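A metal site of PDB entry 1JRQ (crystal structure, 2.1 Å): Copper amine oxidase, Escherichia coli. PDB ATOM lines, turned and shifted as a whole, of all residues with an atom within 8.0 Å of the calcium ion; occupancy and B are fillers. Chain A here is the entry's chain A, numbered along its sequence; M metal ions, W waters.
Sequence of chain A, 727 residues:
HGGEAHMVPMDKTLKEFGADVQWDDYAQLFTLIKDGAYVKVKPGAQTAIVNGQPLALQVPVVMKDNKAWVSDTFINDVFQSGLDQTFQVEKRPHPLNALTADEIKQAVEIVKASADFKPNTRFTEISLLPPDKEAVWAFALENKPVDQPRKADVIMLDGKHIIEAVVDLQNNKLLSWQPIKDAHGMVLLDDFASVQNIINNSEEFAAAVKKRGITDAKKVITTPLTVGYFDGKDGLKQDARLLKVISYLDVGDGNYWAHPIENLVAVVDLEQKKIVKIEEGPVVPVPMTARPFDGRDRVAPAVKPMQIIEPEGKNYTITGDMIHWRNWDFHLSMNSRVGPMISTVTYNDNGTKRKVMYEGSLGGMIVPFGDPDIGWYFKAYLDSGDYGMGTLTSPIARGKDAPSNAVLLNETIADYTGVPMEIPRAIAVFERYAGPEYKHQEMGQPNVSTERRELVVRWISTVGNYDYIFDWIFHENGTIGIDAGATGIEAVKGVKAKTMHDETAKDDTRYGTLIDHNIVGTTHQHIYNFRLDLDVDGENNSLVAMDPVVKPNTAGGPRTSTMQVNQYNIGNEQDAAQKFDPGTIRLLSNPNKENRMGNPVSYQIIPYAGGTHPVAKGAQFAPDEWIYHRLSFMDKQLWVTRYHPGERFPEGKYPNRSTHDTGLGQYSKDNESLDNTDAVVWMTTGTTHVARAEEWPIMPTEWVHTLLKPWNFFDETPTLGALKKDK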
ATOM      1  N   LYS A 133      33.210   6.227   9.756  1.00  0.00           N
ATOM      2  CA  LYS A 133      33.045   4.846  10.210  1.00  0.00           C
ATOM      3  C   LYS A 133      34.032   3.900   9.524  1.00  0.00           C
ATOM      4  O   LYS A 133      34.672   3.079  10.175  1.00  0.00           O
ATOM      5  CB  LYS A 133      31.600   4.432   9.974  1.00  0.00           C
ATOM      6  CG  LYS A 133      31.278   2.956  10.105  1.00  0.00           C
ATOM      7  CD  LYS A 133      29.772   2.700  10.086  1.00  0.00           C
ATOM      8  CE  LYS A 133      29.410   1.237  10.225  1.00  0.00           C
ATOM      9  NZ  LYS A 133      27.981   1.097  10.642  1.00  0.00           N
ATOM     10  N   TRP A 137      36.780   1.596  11.617  1.00  0.00           N
ATOM     11  CA  TRP A 137      36.831   0.139  11.567  1.00  0.00           C
ATOM     12  C   TRP A 137      38.187  -0.361  11.075  1.00  0.00           C
ATOM     13  O   TRP A 137      38.641  -1.377  11.584  1.00  0.00           O
ATOM     14  CB  TRP A 137      35.765  -0.474  10.655  1.00  0.00           C
ATOM     15  CG  TRP A 137      34.475  -0.919  11.285  1.00  0.00           C
ATOM     16  CD1 TRP A 137      33.214  -0.621  10.903  1.00  0.00           C
ATOM     17  CD2 TRP A 137      34.348  -1.781  12.429  1.00  0.00           C
ATOM     18  NE1 TRP A 137      32.289  -1.238  11.723  1.00  0.00           N
ATOM     19  CE2 TRP A 137      32.981  -1.955  12.673  1.00  0.00           C
ATOM     20  CE3 TRP A 137      35.279  -2.422  13.259  1.00  0.00           C
ATOM     21  CZ2 TRP A 137      32.510  -2.736  13.732  1.00  0.00           C
ATOM     22  CZ3 TRP A 137      34.836  -3.203  14.302  1.00  0.00           C
ATOM     23  CH2 TRP A 137      33.462  -3.344  14.514  1.00  0.00           C
ATOM     24  N   VAL A 356      30.648  -6.978  15.027  1.00  0.00           N
ATOM     25  CA  VAL A 356      29.376  -7.250  15.683  1.00  0.00           C
ATOM     26  C   VAL A 356      28.653  -5.911  15.773  1.00  0.00           C
ATOM     27  O   VAL A 356      27.534  -5.788  15.282  1.00  0.00           O
ATOM     28  CB  VAL A 356      29.471  -7.923  17.069  1.00  0.00           C
ATOM     29  CG1 VAL A 356      28.129  -7.994  17.774  1.00  0.00           C
ATOM     30  CG2 VAL A 356      30.113  -9.298  16.925  1.00  0.00           C
ATOM     31  N   MET A 357      29.317  -4.931  16.384  1.00  0.00           N
ATOM     32  CA  MET A 357      28.693  -3.614  16.508  1.00  0.00           C
ATOM     33  C   MET A 357      29.637  -2.429  16.387  1.00  0.00           C
ATOM     34  O   MET A 357      30.657  -2.305  17.076  1.00  0.00           O
ATOM     35  CB  MET A 357      27.933  -3.566  17.842  1.00  0.00           C
ATOM     36  CG  MET A 357      27.121  -2.291  18.045  1.00  0.00           C
ATOM     37  SD  MET A 357      26.098  -2.289  19.528  1.00  0.00           S
ATOM     38  CE  MET A 357      27.320  -2.264  20.838  1.00  0.00           C
ATOM     39  N   TYR A 358      29.285  -1.506  15.479  1.00  0.00           N
ATOM     40  CA  TYR A 358      30.112  -0.324  15.289  1.00  0.00           C
ATOM     41  C   TYR A 358      30.016   0.601  16.497  1.00  0.00           C
ATOM     42  O   TYR A 358      31.021   1.014  17.073  1.00  0.00           O
ATOM     43  CB  TYR A 358      29.785   0.435  14.006  1.00  0.00           C
ATOM     44  CG  TYR A 358      30.710   1.641  13.895  1.00  0.00           C
ATOM     45  CD1 TYR A 358      32.084   1.465  13.799  1.00  0.00           C
ATOM     46  CD2 TYR A 358      30.190   2.923  13.898  1.00  0.00           C
ATOM     47  CE1 TYR A 358      32.920   2.570  13.706  1.00  0.00           C
ATOM     48  CE2 TYR A 358      31.009   4.036  13.817  1.00  0.00           C
ATOM     49  CZ  TYR A 358      32.372   3.845  13.714  1.00  0.00           C
ATOM     50  OH  TYR A 358      33.191   4.950  13.620  1.00  0.00           O
ATOM     51  N   GLU A 359      28.803   0.951  16.914  1.00  0.00           N
ATOM     52  CA  GLU A 359      28.614   1.840  18.060  1.00  0.00           C
ATOM     53  C   GLU A 359      27.251   1.519  18.680  1.00  0.00           C
ATOM     54  O   GLU A 359      26.280   1.280  17.958  1.00  0.00           O
ATOM     55  CB  GLU A 359      28.517   3.317  17.674  1.00  0.00           C
ATOM     56  CG  GLU A 359      29.690   3.957  16.952  1.00  0.00           C
ATOM     57  CD  GLU A 359      29.439   5.421  16.643  1.00  0.00           C
ATOM     58  OE1 GLU A 359      29.991   6.298  17.341  1.00  0.00           O
ATOM     59  OE2 GLU A 359      28.712   5.782  15.690  1.00  0.00           O
ATOM     60  N   ARG A 531      20.265   2.882  20.769  1.00  0.00           N
ATOM     61  CA  ARG A 531      20.696   3.024  19.378  1.00  0.00           C
ATOM     62  C   ARG A 531      21.862   2.055  19.209  1.00  0.00           C
ATOM     63  O   ARG A 531      22.943   2.236  19.790  1.00  0.00           O
ATOM     64  CB  ARG A 531      21.097   4.458  19.036  1.00  0.00           C
ATOM     65  CG  ARG A 531      21.712   4.592  17.652  1.00  0.00           C
ATOM     66  CD  ARG A 531      22.178   6.016  17.343  1.00  0.00           C
ATOM     67  NE  ARG A 531      22.784   6.106  16.016  1.00  0.00           N
ATOM     68  CZ  ARG A 531      23.951   5.604  15.661  1.00  0.00           C
ATOM     69  NH1 ARG A 531      24.681   4.948  16.560  1.00  0.00           N
ATOM     70  NH2 ARG A 531      24.418   5.717  14.419  1.00  0.00           N
ATOM     71  N   LEU A 532      21.626   1.011  18.423  1.00  0.00           N
ATOM     72  CA  LEU A 532      22.614  -0.016  18.146  1.00  0.00           C
ATOM     73  C   LEU A 532      23.007  -0.171  16.684  1.00  0.00           C
ATOM     74  O   LEU A 532      22.376  -0.820  15.846  1.00  0.00           O
ATOM     75  CB  LEU A 532      22.079  -1.342  18.729  1.00  0.00           C
ATOM     76  CG  LEU A 532      21.438  -1.193  20.116  1.00  0.00           C
ATOM     77  CD1 LEU A 532      20.620  -2.423  20.510  1.00  0.00           C
ATOM     78  CD2 LEU A 532      22.528  -0.944  21.175  1.00  0.00           C
ATOM     79  N   ASP A 533      24.144   0.455  16.340  1.00  0.00           N
ATOM     80  CA  ASP A 533      24.622   0.359  14.959  1.00  0.00           C
ATOM     81  C   ASP A 533      25.322  -0.993  14.817  1.00  0.00           C
ATOM     82  O   ASP A 533      26.538  -1.128  14.768  1.00  0.00           O
ATOM     83  CB  ASP A 533      25.523   1.537  14.602  1.00  0.00           C
ATOM     84  CG  ASP A 533      26.093   1.435  13.200  1.00  0.00           C
ATOM     85  OD1 ASP A 533      25.554   0.658  12.408  1.00  0.00           O
ATOM     86  OD2 ASP A 533      27.079   2.088  12.810  1.00  0.00           O
ATOM     87  N   LEU A 534      24.510  -2.048  14.730  1.00  0.00           N
ATOM     88  CA  LEU A 534      25.036  -3.391  14.589  1.00  0.00           C
ATOM     89  C   LEU A 534      25.586  -3.566  13.177  1.00  0.00           C
ATOM     90  O   LEU A 534      24.896  -3.078  12.291  1.00  0.00           O
ATOM     91  CB  LEU A 534      23.910  -4.436  14.758  1.00  0.00           C
ATOM     92  CG  LEU A 534      23.339  -4.489  16.180  1.00  0.00           C
ATOM     93  CD1 LEU A 534      22.120  -5.407  16.192  1.00  0.00           C
ATOM     94  CD2 LEU A 534      24.415  -4.927  17.173  1.00  0.00           C
ATOM     95  N   ASP A 535      26.707  -4.213  12.982  1.00  0.00           N
ATOM     96  CA  ASP A 535      27.312  -4.454  11.686  1.00  0.00           C
ATOM     97  C   ASP A 535      27.529  -5.978  11.803  1.00  0.00           C
ATOM     98  O   ASP A 535      28.605  -6.422  12.199  1.00  0.00           O
ATOM     99  CB  ASP A 535      28.633  -3.751  11.428  1.00  0.00           C
ATOM    100  CG  ASP A 535      28.531  -2.265  11.148  1.00  0.00           C
ATOM    101  OD1 ASP A 535      27.459  -1.713  10.859  1.00  0.00           O
ATOM    102  OD2 ASP A 535      29.555  -1.561  11.197  1.00  0.00           O
ATOM    103  N   VAL A 536      26.504  -6.755  11.478  1.00  0.00           N
ATOM    104  CA  VAL A 536      26.655  -8.202  11.595  1.00  0.00           C
ATOM    105  C   VAL A 536      27.680  -8.813  10.660  1.00  0.00           C
ATOM    106  O   VAL A 536      27.340  -9.061   9.488  1.00  0.00           O
ATOM    107  CB  VAL A 536      25.296  -8.923  11.485  1.00  0.00           C
ATOM    108  CG1 VAL A 536      25.484 -10.430  11.643  1.00  0.00           C
ATOM    109  CG2 VAL A 536      24.331  -8.359  12.513  1.00  0.00           C
ATOM    110  N   GLY A 538      29.836  -7.527   9.193  1.00  0.00           N
ATOM    111  CA  GLY A 538      30.044  -6.694   8.009  1.00  0.00           C
ATOM    112  C   GLY A 538      29.021  -5.562   8.025  1.00  0.00           C
ATOM    113  O   GLY A 538      28.072  -5.586   8.805  1.00  0.00           O
ATOM    114  N   GLU A 539      29.240  -4.589   7.157  1.00  0.00           N
ATOM    115  CA  GLU A 539      28.348  -3.441   7.043  1.00  0.00           C
ATOM    116  C   GLU A 539      26.975  -3.719   6.447  1.00  0.00           C
ATOM    117  O   GLU A 539      25.907  -3.372   6.953  1.00  0.00           O
ATOM    118  CB  GLU A 539      29.022  -2.463   6.064  1.00  0.00           C
ATOM    119  CG  GLU A 539      28.297  -1.135   5.922  1.00  0.00           C
ATOM    120  CD  GLU A 539      28.909  -0.211   4.903  1.00  0.00           C
ATOM    121  OE1 GLU A 539      30.027   0.303   5.101  1.00  0.00           O
ATOM    122  OE2 GLU A 539      28.334   0.061   3.842  1.00  0.00           O
ATOM    123  N   ASN A 540      26.965  -4.380   5.297  1.00  0.00           N
ATOM    124  CA  ASN A 540      25.731  -4.697   4.592  1.00  0.00           C
ATOM    125  C   ASN A 540      24.883  -5.822   5.154  1.00  0.00           C
ATOM    126  O   ASN A 540      25.259  -6.982   5.057  1.00  0.00           O
ATOM    127  CB  ASN A 540      26.072  -4.899   3.110  1.00  0.00           C
ATOM    128  CG  ASN A 540      26.778  -3.672   2.554  1.00  0.00           C
ATOM    129  OD1 ASN A 540      26.434  -2.529   2.869  1.00  0.00           O
ATOM    130  ND2 ASN A 540      27.797  -3.848   1.723  1.00  0.00           N
ATOM    131  N   ASN A 541      23.747  -5.477   5.747  1.00  0.00           N
ATOM    132  CA  ASN A 541      22.843  -6.453   6.334  1.00  0.00           C
ATOM    133  C   ASN A 541      21.403  -6.223   5.894  1.00  0.00           C
ATOM    134  O   ASN A 541      21.076  -5.246   5.207  1.00  0.00           O
ATOM    135  CB  ASN A 541      22.885  -6.320   7.867  1.00  0.00           C
ATOM    136  CG  ASN A 541      24.268  -6.353   8.488  1.00  0.00           C
ATOM    137  OD1 ASN A 541      25.213  -6.992   8.011  1.00  0.00           O
ATOM    138  ND2 ASN A 541      24.397  -5.633   9.608  1.00  0.00           N
ATOM    139  N   LEU A 588      18.860  -9.555  12.209  1.00  0.00           N
ATOM    140  CA  LEU A 588      19.618  -8.569  11.458  1.00  0.00           C
ATOM    141  C   LEU A 588      20.602  -9.580  10.860  1.00  0.00           C
ATOM    142  O   LEU A 588      21.470 -10.105  11.567  1.00  0.00           O
ATOM    143  CB  LEU A 588      20.272  -7.414  12.223  1.00  0.00           C
ATOM    144  CG  LEU A 588      21.022  -6.450  11.298  1.00  0.00           C
ATOM    145  CD1 LEU A 588      20.038  -5.831  10.310  1.00  0.00           C
ATOM    146  CD2 LEU A 588      21.782  -5.352  12.017  1.00  0.00           C
ATOM    147  N   VAL A 640      14.608   0.298  12.518  1.00  0.00           N
ATOM    148  CA  VAL A 640      15.834   0.002  11.790  1.00  0.00           C
ATOM    149  C   VAL A 640      15.913   1.127  10.756  1.00  0.00           C
ATOM    150  O   VAL A 640      14.922   1.357  10.054  1.00  0.00           O
ATOM    151  CB  VAL A 640      15.921  -1.371  11.115  1.00  0.00           C
ATOM    152  CG1 VAL A 640      17.278  -1.577  10.472  1.00  0.00           C
ATOM    153  CG2 VAL A 640      15.627  -2.500  12.098  1.00  0.00           C
ATOM    154  N   THR A 641      17.058   1.811  10.682  1.00  0.00           N
ATOM    155  CA  THR A 641      17.151   2.899   9.708  1.00  0.00           C
ATOM    156  C   THR A 641      18.499   2.759   9.019  1.00  0.00           C
ATOM    157  O   THR A 641      19.304   1.959   9.503  1.00  0.00           O
ATOM    158  CB  THR A 641      17.133   4.282  10.394  1.00  0.00           C
ATOM    159  OG1 THR A 641      18.256   4.363  11.303  1.00  0.00           O
ATOM    160  CG2 THR A 641      15.860   4.469  11.205  1.00  0.00           C
ATOM    161  N   ARG A 642      18.671   3.530   7.947  1.00  0.00           N
ATOM    162  CA  ARG A 642      19.934   3.489   7.206  1.00  0.00           C
ATOM    163  C   ARG A 642      20.960   4.252   8.056  1.00  0.00           C
ATOM    164  O   ARG A 642      20.553   5.269   8.604  1.00  0.00           O
ATOM    165  CB  ARG A 642      19.792   4.236   5.881  1.00  0.00           C
ATOM    166  CG  ARG A 642      18.876   3.583   4.844  1.00  0.00           C
ATOM    167  CD  ARG A 642      19.463   3.881   3.467  1.00  0.00           C
ATOM    168  NE  ARG A 642      19.315   2.745   2.565  1.00  0.00           N
ATOM    169  CZ  ARG A 642      20.095   2.537   1.523  1.00  0.00           C
ATOM    170  NH1 ARG A 642      21.076   3.401   1.288  1.00  0.00           N
ATOM    171  NH2 ARG A 642      19.866   1.475   0.767  1.00  0.00           N
ATOM    172  N   TYR A 643      22.184   3.751   8.131  1.00  0.00           N
ATOM    173  CA  TYR A 643      23.223   4.416   8.911  1.00  0.00           C
ATOM    174  C   TYR A 643      23.415   5.845   8.425  1.00  0.00           C
ATOM    175  O   TYR A 643      23.563   6.029   7.225  1.00  0.00           O
ATOM    176  CB  TYR A 643      24.567   3.686   8.742  1.00  0.00           C
ATOM    177  CG  TYR A 643      25.704   4.487   9.326  1.00  0.00           C
ATOM    178  CD1 TYR A 643      25.807   4.659  10.704  1.00  0.00           C
ATOM    179  CD2 TYR A 643      26.664   5.084   8.519  1.00  0.00           C
ATOM    180  CE1 TYR A 643      26.824   5.398  11.269  1.00  0.00           C
ATOM    181  CE2 TYR A 643      27.693   5.824   9.093  1.00  0.00           C
ATOM    182  CZ  TYR A 643      27.762   5.973  10.460  1.00  0.00           C
ATOM    183  OH  TYR A 643      28.779   6.712  11.026  1.00  0.00           O
ATOM    184  N   THR A 677      22.153  -3.313   3.221  1.00  0.00           N
ATOM    185  CA  THR A 677      22.819  -2.007   3.400  1.00  0.00           C
ATOM    186  C   THR A 677      23.176  -1.792   4.854  1.00  0.00           C
ATOM    187  O   THR A 677      22.807  -2.608   5.706  1.00  0.00           O
ATOM    188  CB  THR A 677      21.849  -0.955   2.836  1.00  0.00           C
ATOM    189  OG1 THR A 677      22.536   0.269   2.607  1.00  0.00           O
ATOM    190  CG2 THR A 677      20.653  -0.770   3.761  1.00  0.00           C
ATOM    191  N   ASP A 678      23.903  -0.727   5.174  1.00  0.00           N
ATOM    192  CA  ASP A 678      24.302  -0.440   6.544  1.00  0.00           C
ATOM    193  C   ASP A 678      23.105  -0.068   7.409  1.00  0.00           C
ATOM    194  O   ASP A 678      22.601   1.052   7.335  1.00  0.00           O
ATOM    195  CB  ASP A 678      25.365   0.660   6.560  1.00  0.00           C
ATOM    196  CG  ASP A 678      26.035   0.812   7.906  1.00  0.00           C
ATOM    197  OD1 ASP A 678      25.454   0.341   8.895  1.00  0.00           O
ATOM    198  OD2 ASP A 678      27.132   1.410   8.011  1.00  0.00           O
ATOM    199  N   ALA A 679      22.600  -0.967   8.257  1.00  0.00           N
ATOM    200  CA  ALA A 679      21.451  -0.687   9.101  1.00  0.00           C
ATOM    201  C   ALA A 679      21.796  -0.283  10.535  1.00  0.00           C
ATOM    202  O   ALA A 679      22.847  -0.633  11.054  1.00  0.00           O
ATOM    203  CB  ALA A 679      20.585  -1.937   9.267  1.00  0.00           C
ATOM    204  N   VAL A 680      20.896   0.449  11.172  1.00  0.00           N
ATOM    205  CA  VAL A 680      21.095   0.880  12.552  1.00  0.00           C
ATOM    206  C   VAL A 680      19.823   0.443  13.279  1.00  0.00           C
ATOM    207  O   VAL A 680      18.747   0.871  12.861  1.00  0.00           O
ATOM    208  CB  VAL A 680      21.309   2.391  12.722  1.00  0.00           C
ATOM    209  CG1 VAL A 680      21.541   2.731  14.192  1.00  0.00           C
ATOM    210  CG2 VAL A 680      22.527   2.848  11.921  1.00  0.00           C
ATOM    211  N   VAL A 681      19.947  -0.370  14.315  1.00  0.00           N
ATOM    212  CA  VAL A 681      18.792  -0.851  15.065  1.00  0.00           C
ATOM    213  C   VAL A 681      18.496   0.011  16.271  1.00  0.00           C
ATOM    214  O   VAL A 681      19.427   0.424  16.967  1.00  0.00           O
ATOM    215  CB  VAL A 681      19.040  -2.295  15.541  1.00  0.00           C
ATOM    216  CG1 VAL A 681      17.916  -2.798  16.435  1.00  0.00           C
ATOM    217  CG2 VAL A 681      19.222  -3.217  14.332  1.00  0.00           C
HETATM  218 CA    CA M   1      25.158  -1.109  10.822  1.00  0.00          CA
HETATM  219  O   HOH W   1      24.629  -3.077   9.168  1.00  0.00           O
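The side-chain amino group (NZ) of Lys 133 lies within salt-bridge range of the side-chain carboxylate (OD2) of Asp 535, 3.1 Å away.
The backbone carbonyl oxygen (O) of Val 356 sits at hydrogen-bond distance from the backbone NH (N) of Asp 535, 2.9 Å away.
OD2 of Asp 535 sits at hydrogen-bond distance from NE1 of Trp 137 (2.8 Å).
NZ of Lys 133 lies within salt-bridge range of OD2 of Asp 533, at 2.5 Å.
O of Asp 533 lies within hydrogen-bond range of N of Tyr 358.
O of Glu 359 is in hydrogen-bond range of N of Asp 533 (2.8 Å).
The side-chain amino group of Lys 133 is in salt-bridge range of the side-chain carboxylate of Asp 678 (2.8 Å).
The backbone carbonyl oxygen of Asp 678 sits at hydrogen-bond distance from the backbone NH of Tyr 643, at 2.8 Å.
Lys 133 touches the calcium ion (NZ to CA, 3.6 Å).
Six residues have an atom within 4 Å of the calcium ion: Lys 133, Asp 533, Leu 534, Asp 535, Asp 678 and Ala 679.
The calcium ion is bound by the backbone carbonyl oxygen (O) of Ala 679, the side-chain carboxylate (OD1) of Asp 535, the side-chain carboxylate (OD1) of Asp 533, the side-chain carboxylate (OD1) of Asp 678, the backbone carbonyl oxygen (O) of Leu 534 and water W1.
Water W1 lies within hydrogen-bond range of O of Glu 539 (2.6 Å), ND2 of Asn 541 (2.6 Å) and N of Ala 679 (3.1 Å).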
